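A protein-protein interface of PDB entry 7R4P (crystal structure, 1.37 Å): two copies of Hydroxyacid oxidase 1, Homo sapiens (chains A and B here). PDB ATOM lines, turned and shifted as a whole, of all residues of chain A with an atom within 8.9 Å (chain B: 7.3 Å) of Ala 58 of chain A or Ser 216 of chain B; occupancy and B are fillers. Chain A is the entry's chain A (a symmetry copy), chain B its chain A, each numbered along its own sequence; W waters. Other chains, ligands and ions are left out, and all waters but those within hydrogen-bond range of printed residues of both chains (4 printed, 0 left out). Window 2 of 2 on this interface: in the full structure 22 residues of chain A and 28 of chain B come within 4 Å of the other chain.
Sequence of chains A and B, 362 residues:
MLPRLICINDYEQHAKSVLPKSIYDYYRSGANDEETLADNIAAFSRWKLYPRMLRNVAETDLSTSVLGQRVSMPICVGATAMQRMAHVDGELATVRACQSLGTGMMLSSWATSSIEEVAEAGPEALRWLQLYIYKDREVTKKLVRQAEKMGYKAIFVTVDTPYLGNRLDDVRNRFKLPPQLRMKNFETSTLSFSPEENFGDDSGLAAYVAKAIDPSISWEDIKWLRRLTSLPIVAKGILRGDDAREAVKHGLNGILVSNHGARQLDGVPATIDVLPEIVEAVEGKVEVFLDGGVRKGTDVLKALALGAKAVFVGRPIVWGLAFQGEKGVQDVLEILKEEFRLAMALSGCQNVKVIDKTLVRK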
ATOM      1  N   MET A  53      -3.037  14.429  18.401  1.00  0.00           N
ATOM      2  CA  MET A  53      -4.176  13.731  19.015  1.00  0.00           C
ATOM      3  C   MET A  53      -3.941  13.626  20.521  1.00  0.00           C
ATOM      4  O   MET A  53      -2.773  13.607  21.004  1.00  0.00           O
ATOM      5  CB  MET A  53      -4.359  12.351  18.368  1.00  0.00           C
ATOM      6  CG  MET A  53      -4.500  12.453  16.802  1.00  0.00           C
ATOM      7  SD  MET A  53      -5.828  13.499  16.358  1.00  0.00           S
ATOM      8  CE  MET A  53      -5.408  13.823  14.638  1.00  0.00           C
ATOM      9  N   LEU A  54      -5.019  13.395  21.239  1.00  0.00           N
ATOM     10  CA  LEU A  54      -4.954  12.933  22.637  1.00  0.00           C
ATOM     11  C   LEU A  54      -4.247  13.968  23.547  1.00  0.00           C
ATOM     12  O   LEU A  54      -3.427  13.568  24.405  1.00  0.00           O
ATOM     13  CB  LEU A  54      -4.286  11.568  22.675  1.00  0.00           C
ATOM     14  CG  LEU A  54      -5.020  10.500  21.875  1.00  0.00           C
ATOM     15  CD1 LEU A  54      -4.171   9.273  21.714  1.00  0.00           C
ATOM     16  CD2 LEU A  54      -6.320  10.114  22.491  1.00  0.00           C
ATOM     17  N   ARG A  55      -4.596  15.245  23.405  1.00  0.00           N
ATOM     18  CA  ARG A  55      -3.897  16.308  24.179  1.00  0.00           C
ATOM     19  C   ARG A  55      -4.754  16.921  25.293  1.00  0.00           C
ATOM     20  O   ARG A  55      -4.214  17.777  25.995  1.00  0.00           O
ATOM     21  CB  ARG A  55      -3.489  17.446  23.244  1.00  0.00           C
ATOM     22  CG  ARG A  55      -2.695  17.012  22.024  1.00  0.00           C
ATOM     23  CD  ARG A  55      -1.498  16.214  22.469  1.00  0.00           C
ATOM     24  NE  ARG A  55      -0.346  17.068  22.667  1.00  0.00           N
ATOM     25  CZ  ARG A  55       0.874  16.620  22.924  1.00  0.00           C
ATOM     26  NH1 ARG A  55       1.095  15.321  23.033  1.00  0.00           N
ATOM     27  NH2 ARG A  55       1.865  17.477  23.083  1.00  0.00           N
ATOM     28  N   ASN A  56      -6.005  16.529  25.440  1.00  0.00           N
ATOM     29  CA  ASN A  56      -6.946  17.126  26.441  1.00  0.00           C
ATOM     30  C   ASN A  56      -7.358  18.532  25.996  1.00  0.00           C
ATOM     31  O   ASN A  56      -6.676  19.478  26.343  1.00  0.00           O
ATOM     32  CB  ASN A  56      -6.466  17.120  27.894  1.00  0.00           C
ATOM     33  CG  ASN A  56      -7.565  17.554  28.841  1.00  0.00           C
ATOM     34  OD1 ASN A  56      -8.631  17.986  28.414  1.00  0.00           O
ATOM     35  ND2 ASN A  56      -7.321  17.431  30.133  1.00  0.00           N
ATOM     36  N   VAL A  57      -8.470  18.603  25.282  1.00  0.00           N
ATOM     37  CA  VAL A  57      -8.936  19.902  24.726  1.00  0.00           C
ATOM     38  C   VAL A  57     -10.343  20.171  25.263  1.00  0.00           C
ATOM     39  O   VAL A  57     -11.131  20.813  24.581  1.00  0.00           O
ATOM     40  CB  VAL A  57      -8.843  19.872  23.184  1.00  0.00           C
ATOM     41  CG1 VAL A  57      -7.397  19.888  22.718  1.00  0.00           C
ATOM     42  CG2 VAL A  57      -9.589  18.687  22.589  1.00  0.00           C
ATOM     43  N   ALA A  58     -10.622  19.688  26.477  1.00  0.00           N
ATOM     44  CA  ALA A  58     -11.910  19.960  27.134  1.00  0.00           C
ATOM     45  C   ALA A  58     -12.002  21.434  27.433  1.00  0.00           C
ATOM     46  O   ALA A  58     -13.186  21.945  27.461  1.00  0.00           O
ATOM     47  CB  ALA A  58     -12.009  19.204  28.414  1.00  0.00           C
ATOM     48  N   GLU A  59     -10.904  22.113  27.656  1.00  0.00           N
ATOM     49  CA  GLU A  59     -11.228  23.480  28.152  1.00  0.00           C
ATOM     50  C   GLU A  59     -10.718  24.587  27.251  1.00  0.00           C
ATOM     51  O   GLU A  59     -10.266  25.546  27.815  1.00  0.00           O
ATOM     52  CB  GLU A  59     -10.763  23.643  29.586  1.00  0.00           C
ATOM     53  CG  GLU A  59     -11.799  23.067  30.517  1.00  0.00           C
ATOM     54  N   THR A  60     -10.993  24.576  25.964  1.00  0.00           N
ATOM     55  CA  THR A  60     -10.237  25.396  24.982  1.00  0.00           C
ATOM     56  C   THR A  60     -10.338  26.886  25.306  1.00  0.00           C
ATOM     57  O   THR A  60     -11.457  27.357  25.472  1.00  0.00           O
ATOM     58  CB  THR A  60     -10.804  25.222  23.578  1.00  0.00           C
ATOM     59  OG1 THR A  60     -12.187  25.520  23.712  1.00  0.00           O
ATOM     60  CG2 THR A  60     -10.549  23.837  23.045  1.00  0.00           C
ATOM     61  N   ASP A  61      -9.202  27.547  25.474  1.00  0.00           N
ATOM     62  CA  ASP A  61      -9.117  28.977  25.852  1.00  0.00           C
ATOM     63  C   ASP A  61      -8.651  29.715  24.625  1.00  0.00           C
ATOM     64  O   ASP A  61      -7.485  29.470  24.200  1.00  0.00           O
ATOM     65  CB  ASP A  61      -8.146  29.205  27.023  1.00  0.00           C
ATOM     66  CG  ASP A  61      -7.977  30.638  27.513  1.00  0.00           C
ATOM     67  OD1 ASP A  61      -8.455  31.541  26.892  1.00  0.00           O
ATOM     68  OD2 ASP A  61      -7.296  30.847  28.578  1.00  0.00           O
ATOM     69  N   ARG A 341     -12.269  27.673  17.617  1.00  0.00           N
ATOM     70  CA  ARG A 341     -12.264  26.782  18.807  1.00  0.00           C
ATOM     71  C   ARG A 341     -12.191  25.325  18.348  1.00  0.00           C
ATOM     72  O   ARG A 341     -11.308  24.594  18.813  1.00  0.00           O
ATOM     73  CB  ARG A 341     -13.523  27.018  19.645  1.00  0.00           C
ATOM     74  CG  ARG A 341     -13.582  26.165  20.902  1.00  0.00           C
ATOM     75  CD  ARG A 341     -14.859  26.383  21.688  1.00  0.00           C
ATOM     76  NE  ARG A 341     -15.237  27.787  21.763  1.00  0.00           N
ATOM     77  CZ  ARG A 341     -14.754  28.657  22.644  1.00  0.00           C
ATOM     78  NH1 ARG A 341     -13.863  28.272  23.542  1.00  0.00           N
ATOM     79  NH2 ARG A 341     -15.169  29.910  22.625  1.00  0.00           N
ATOM     80  N   ALA A 345      -9.192  22.655  18.968  1.00  0.00           N
ATOM     81  CA  ALA A 345      -9.459  21.376  19.666  1.00  0.00           C
ATOM     82  C   ALA A 345      -9.056  20.184  18.788  1.00  0.00           C
ATOM     83  O   ALA A 345      -8.383  19.306  19.289  1.00  0.00           O
ATOM     84  CB  ALA A 345     -10.915  21.315  20.041  1.00  0.00           C
ATOM     85  N   GLY A 348      -5.378  19.634  18.749  1.00  0.00           N
ATOM     86  CA  GLY A 348      -4.714  19.291  20.032  1.00  0.00           C
ATOM     87  C   GLY A 348      -4.257  20.494  20.825  1.00  0.00           C
ATOM     88  O   GLY A 348      -3.421  20.335  21.685  1.00  0.00           O
ATOM     89  N   CYS A 349      -4.827  21.647  20.535  1.00  0.00           N
ATOM     90  CA  CYS A 349      -4.379  22.903  21.182  1.00  0.00           C
ATOM     91  C   CYS A 349      -5.407  23.394  22.206  1.00  0.00           C
ATOM     92  O   CYS A 349      -6.506  23.749  21.807  1.00  0.00           O
ATOM     93  CB  CYS A 349      -4.226  23.998  20.137  1.00  0.00           C
ATOM     94  SG  CYS A 349      -2.984  23.600  18.880  1.00  0.00           S
ATOM     95  N   GLN A 350      -5.008  23.425  23.481  1.00  0.00           N
ATOM     96  CA  GLN A 350      -5.980  23.840  24.516  1.00  0.00           C
ATOM     97  C   GLN A 350      -5.976  25.355  24.667  1.00  0.00           C
ATOM     98  O   GLN A 350      -6.994  25.876  25.219  1.00  0.00           O
ATOM     99  CB  GLN A 350      -5.637  23.219  25.860  1.00  0.00           C
ATOM    100  N   ASN A 351      -4.977  26.060  24.182  1.00  0.00           N
ATOM    101  CA  ASN A 351      -4.880  27.539  24.308  1.00  0.00           C
ATOM    102  C   ASN A 351      -4.000  28.081  23.197  1.00  0.00           C
ATOM    103  O   ASN A 351      -3.344  27.274  22.463  1.00  0.00           O
ATOM    104  CB  ASN A 351      -4.384  27.945  25.704  1.00  0.00           C
ATOM    105  CG  ASN A 351      -2.971  27.468  25.970  1.00  0.00           C
ATOM    106  OD1 ASN A 351      -2.031  27.804  25.247  1.00  0.00           O
ATOM    107  ND2 ASN A 351      -2.847  26.621  26.961  1.00  0.00           N
ATOM    108  N   ILE B 133     -13.567   6.464  23.407  1.00  0.00           N
ATOM    109  CA  ILE B 133     -13.563   6.604  24.899  1.00  0.00           C
ATOM    110  C   ILE B 133     -14.613   7.636  25.320  1.00  0.00           C
ATOM    111  O   ILE B 133     -14.373   8.849  25.242  1.00  0.00           O
ATOM    112  CB  ILE B 133     -12.147   6.793  25.478  1.00  0.00           C
ATOM    113  CG1 ILE B 133     -11.226   5.679  24.968  1.00  0.00           C
ATOM    114  CG2 ILE B 133     -12.186   6.919  27.010  1.00  0.00           C
ATOM    115  CD1 ILE B 133      -9.831   5.757  25.536  1.00  0.00           C
ATOM    116  N   LYS B 135     -17.298   9.730  27.843  1.00  0.00           N
ATOM    117  CA  LYS B 135     -17.169  10.330  29.196  1.00  0.00           C
ATOM    118  C   LYS B 135     -17.536   9.236  30.204  1.00  0.00           C
ATOM    119  O   LYS B 135     -16.877   9.137  31.219  1.00  0.00           O
ATOM    120  CB  LYS B 135     -18.113  11.516  29.292  1.00  0.00           C
ATOM    121  CG  LYS B 135     -17.740  12.721  28.438  1.00  0.00           C
ATOM    122  CD  LYS B 135     -18.805  13.787  28.493  1.00  0.00           C
ATOM    123  CE  LYS B 135     -18.588  14.924  27.522  1.00  0.00           C
ATOM    124  NZ  LYS B 135     -19.760  15.828  27.489  1.00  0.00           N
ATOM    125  N   ARG B 137     -17.021   5.959  31.327  1.00  0.00           N
ATOM    126  CA  ARG B 137     -16.007   4.894  31.161  1.00  0.00           C
ATOM    127  C   ARG B 137     -16.618   3.519  31.467  1.00  0.00           C
ATOM    128  O   ARG B 137     -16.043   2.526  31.076  1.00  0.00           O
ATOM    129  CB  ARG B 137     -14.822   5.161  32.082  1.00  0.00           C
ATOM    130  CG  ARG B 137     -14.073   6.441  31.748  1.00  0.00           C
ATOM    131  CD  ARG B 137     -13.359   6.392  30.410  1.00  0.00           C
ATOM    132  NE  ARG B 137     -12.293   7.379  30.420  1.00  0.00           N
ATOM    133  CZ  ARG B 137     -12.461   8.659  30.122  1.00  0.00           C
ATOM    134  NH1 ARG B 137     -13.650   9.101  29.755  1.00  0.00           N
ATOM    135  NH2 ARG B 137     -11.436   9.486  30.181  1.00  0.00           N
ATOM    136  N   PRO B 162     -12.159  14.422  19.535  1.00  0.00           N
ATOM    137  CA  PRO B 162     -12.550  15.001  20.816  1.00  0.00           C
ATOM    138  C   PRO B 162     -13.900  15.711  20.763  1.00  0.00           C
ATOM    139  O   PRO B 162     -14.569  15.845  21.760  1.00  0.00           O
ATOM    140  CB  PRO B 162     -11.436  15.944  21.180  1.00  0.00           C
ATOM    141  CG  PRO B 162     -10.858  16.341  19.792  1.00  0.00           C
ATOM    142  CD  PRO B 162     -10.978  15.090  18.970  1.00  0.00           C
ATOM    143  N   TYR B 163     -14.173  16.301  19.603  1.00  0.00           N
ATOM    144  CA  TYR B 163     -15.453  16.906  19.170  1.00  0.00           C
ATOM    145  C   TYR B 163     -15.702  16.412  17.758  1.00  0.00           C
ATOM    146  O   TYR B 163     -14.729  16.048  17.057  1.00  0.00           O
ATOM    147  CB  TYR B 163     -15.375  18.438  19.168  1.00  0.00           C
ATOM    148  CG  TYR B 163     -15.097  19.033  20.524  1.00  0.00           C
ATOM    149  CD1 TYR B 163     -16.106  19.296  21.457  1.00  0.00           C
ATOM    150  CD2 TYR B 163     -13.795  19.344  20.941  1.00  0.00           C
ATOM    151  CE1 TYR B 163     -15.825  19.818  22.689  1.00  0.00           C
ATOM    152  CE2 TYR B 163     -13.508  19.856  22.191  1.00  0.00           C
ATOM    153  CZ  TYR B 163     -14.522  20.084  23.100  1.00  0.00           C
ATOM    154  OH  TYR B 163     -14.267  20.634  24.321  1.00  0.00           O
ATOM    155  N   ILE B 213     -19.177  11.981  23.892  1.00  0.00           N
ATOM    156  CA  ILE B 213     -17.745  11.778  23.607  1.00  0.00           C
ATOM    157  C   ILE B 213     -16.923  12.752  24.483  1.00  0.00           C
ATOM    158  O   ILE B 213     -17.295  13.932  24.661  1.00  0.00           O
ATOM    159  CB  ILE B 213     -17.442  11.990  22.122  1.00  0.00           C
ATOM    160  CG1 ILE B 213     -18.133  10.983  21.194  1.00  0.00           C
ATOM    161  CG2 ILE B 213     -15.984  11.851  21.953  1.00  0.00           C
ATOM    162  CD1 ILE B 213     -18.631   9.702  21.850  1.00  0.00           C
ATOM    163  N   ASP B 214     -15.843  12.209  25.033  1.00  0.00           N
ATOM    164  CA  ASP B 214     -14.982  12.913  25.984  1.00  0.00           C
ATOM    165  C   ASP B 214     -13.930  13.765  25.269  1.00  0.00           C
ATOM    166  O   ASP B 214     -12.965  13.244  24.755  1.00  0.00           O
ATOM    167  CB  ASP B 214     -14.413  11.949  26.990  1.00  0.00           C
ATOM    168  CG  ASP B 214     -13.802  12.615  28.185  1.00  0.00           C
ATOM    169  OD1 ASP B 214     -13.528  13.833  28.194  1.00  0.00           O
ATOM    170  OD2 ASP B 214     -13.607  11.874  29.183  1.00  0.00           O
ATOM    171  N   PRO B 215     -13.975  15.095  25.393  1.00  0.00           N
ATOM    172  CA  PRO B 215     -12.892  15.877  24.765  1.00  0.00           C
ATOM    173  C   PRO B 215     -11.593  15.932  25.568  1.00  0.00           C
ATOM    174  O   PRO B 215     -10.628  16.445  25.056  1.00  0.00           O
ATOM    175  CB  PRO B 215     -13.510  17.262  24.662  1.00  0.00           C
ATOM    176  CG  PRO B 215     -14.430  17.360  25.899  1.00  0.00           C
ATOM    177  CD  PRO B 215     -15.013  15.940  26.021  1.00  0.00           C
ATOM    178  N   SER B 216     -11.572  15.389  26.770  1.00  0.00           N
ATOM    179  CA  SER B 216     -10.403  15.388  27.677  1.00  0.00           C
ATOM    180  C   SER B 216      -9.467  14.193  27.417  1.00  0.00           C
ATOM    181  O   SER B 216      -8.438  14.149  28.117  1.00  0.00           O
ATOM    182  CB  SER B 216     -10.836  15.470  29.125  1.00  0.00           C
ATOM    183  OG  SER B 216     -11.350  14.208  29.538  1.00  0.00           O
ATOM    184  N   ILE B 217      -9.793  13.313  26.526  1.00  0.00           N
ATOM    185  CA  ILE B 217      -8.996  12.072  26.372  1.00  0.00           C
ATOM    186  C   ILE B 217      -7.529  12.429  26.101  1.00  0.00           C
ATOM    187  O   ILE B 217      -7.177  13.328  25.253  1.00  0.00           O
ATOM    188  CB  ILE B 217      -9.578  11.152  25.296  1.00  0.00           C
ATOM    189  CG1 ILE B 217     -10.975  10.688  25.709  1.00  0.00           C
ATOM    190  CG2 ILE B 217      -8.703   9.910  25.060  1.00  0.00           C
ATOM    191  CD1 ILE B 217     -11.060  10.187  27.087  1.00  0.00           C
ATOM    192  N   SER B 218      -6.657  11.741  26.790  1.00  0.00           N
ATOM    193  CA  SER B 218      -5.202  11.940  26.672  1.00  0.00           C
ATOM    194  C   SER B 218      -4.549  10.585  26.535  1.00  0.00           C
ATOM    195  O   SER B 218      -5.219   9.528  26.582  1.00  0.00           O
ATOM    196  CB  SER B 218      -4.643  12.679  27.851  1.00  0.00           C
ATOM    197  OG  SER B 218      -4.557  11.853  28.986  1.00  0.00           O
ATOM    198  N   TRP B 219      -3.254  10.591  26.400  1.00  0.00           N
ATOM    199  CA  TRP B 219      -2.449   9.345  26.429  1.00  0.00           C
ATOM    200  C   TRP B 219      -2.648   8.602  27.749  1.00  0.00           C
ATOM    201  O   TRP B 219      -2.494   7.352  27.727  1.00  0.00           O
ATOM    202  CB  TRP B 219      -0.973   9.653  26.142  1.00  0.00           C
ATOM    203  CG  TRP B 219      -0.742  10.116  24.736  1.00  0.00           C
ATOM    204  CD1 TRP B 219      -0.541  11.401  24.270  1.00  0.00           C
ATOM    205  CD2 TRP B 219      -0.797   9.282  23.570  1.00  0.00           C
ATOM    206  NE1 TRP B 219      -0.404  11.375  22.913  1.00  0.00           N
ATOM    207  CE2 TRP B 219      -0.588  10.108  22.437  1.00  0.00           C
ATOM    208  CE3 TRP B 219      -1.005   7.918  23.371  1.00  0.00           C
ATOM    209  CZ2 TRP B 219      -0.517   9.587  21.150  1.00  0.00           C
ATOM    210  CZ3 TRP B 219      -0.947   7.416  22.109  1.00  0.00           C
ATOM    211  CH2 TRP B 219      -0.710   8.241  21.008  1.00  0.00           C
ATOM    212  N   ASP B 221      -5.463   8.019  29.110  1.00  0.00           N
ATOM    213  CA  ASP B 221      -6.660   7.198  28.795  1.00  0.00           C
ATOM    214  C   ASP B 221      -6.285   6.009  27.901  1.00  0.00           C
ATOM    215  O   ASP B 221      -6.944   4.956  27.986  1.00  0.00           O
ATOM    216  CB  ASP B 221      -7.799   8.046  28.278  1.00  0.00           C
ATOM    217  CG  ASP B 221      -8.117   9.110  29.277  1.00  0.00           C
ATOM    218  OD1 ASP B 221      -8.583   8.757  30.363  1.00  0.00           O
ATOM    219  OD2 ASP B 221      -7.878  10.304  29.013  1.00  0.00           O
HETATM  220  O   HOH W   1      -7.261  14.323  30.564  1.00  0.00           O
HETATM  221  O   HOH W   2      -0.156  13.723  21.022  1.00  0.00           O
HETATM  222  O   HOH W   3     -13.623  23.310  23.856  1.00  0.00           O
HETATM  223  O   HOH W   4      -8.571  15.043  23.734  1.00  0.00           O
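No position is printed for both chains.
The backbone NH (N) of Asn 56 of chain A sits at hydrogen-bond distance from the backbone carbonyl oxygen (O) of Ile 217 of chain B (3.4 Å). The backbone carbonyl oxygen (O) of Val 57 of chain A lies within hydrogen-bond range of the side-chain hydroxyl (OH) of Tyr 163 of chain B (3.2 Å). O of Pro 215 of chain B lies within hydrogen-bond range of N of Val 57 of chain A, at 3.1 Å.
Among the printed residues, no Asp or Glu carboxylate lies within 4 Å of a Lys or Arg side-chain nitrogen of the other chain.
The backbone NH (N) of Ser 218 of chain B is in hydrogen-bond range of the side-chain carboxylate (OD2) of Asp 221 of chain B (2.9 Å). The side-chain carboxylate of Asp 214 of chain B sits at hydrogen-bond distance from the side-chain hydroxyl of Ser 216 of chain B. N of Ala 58 of chain A sits at hydrogen-bond distance from OD1 of Asn 56 of chain A (3.3 Å).
Printed residues of chain B within 4 Å of Leu 54 of chain A: Ile 217, Ser 218 and Trp 219. Printed residues of chain B within 4 Å of Asn 56 of chain A: Pro 215, Ser 216 and Ile 217. Of the printed residues of chain B, Val 57 of chain A touches Pro 162, Tyr 163 and Pro 215. Ala 58 of chain A touches three residues of chain B. Of the printed residues of chain A, Tyr 163 of chain B touches Val 57, Ala 58 and Ala 345. Of chain A, only Asn 56 (3.2 Å) and Ala 58 (3.98 Å) come within 4 Å of Ser 216 of chain B. The nearest residue of chain A that does not touch Ser 216 of chain B is Val 57 of chain A (4.5 Å).
Water W2 lies within hydrogen-bond range of the backbone carbonyl oxygen (O) of Met 53 of chain A (2.6 Å), the guanidinium group (NH1) of Arg 55 of chain A (2.9 Å) and the indole nitrogen (NE1) of Trp 219 of chain B (3.0 Å). Water W3 lies within hydrogen-bond range of OG1 of Thr 60 of chain A (2.6 Å) and OH of Tyr 163 of chain B (2.8 Å). Water W4 lies within hydrogen-bond range of O of Ile 217 of chain B (2.7 Å), O of Pro 215 of chain B (2.8 Å) and N of Asn 56 of chain A (3.4 Å). Water W1 bridges the backbone carbonyl oxygen of Ser 216 of chain B (2.7 Å) and the side-chain amide nitrogen of Asn 56 of chain A (3.1 Å).
Met 53 of chain A touches Trp 219 of chain B. Ile 217 of chain B touches Leu 54 of chain A. Leu 54 of chain A touches Ser 218 of chain B (O to CA, 3.3 Å). Leu 54 of chain A touches Trp 219 of chain B (O to N, 3.6 Å). Pro 215 of chain B touches Asn 56 of chain A (O to C, 3.99 Å). Ser 216 of chain B touches Asn 56 of chain A (CA to OD1, 3.2 Å). Val 57 of chain A touches Pro 162 of chain B. Ala 58 of chain A touches Pro 215 of chain B. Ala 345 of chain A touches Pro 162 of chain B. Ala 345 of chain A touches Tyr 163 of chain B.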
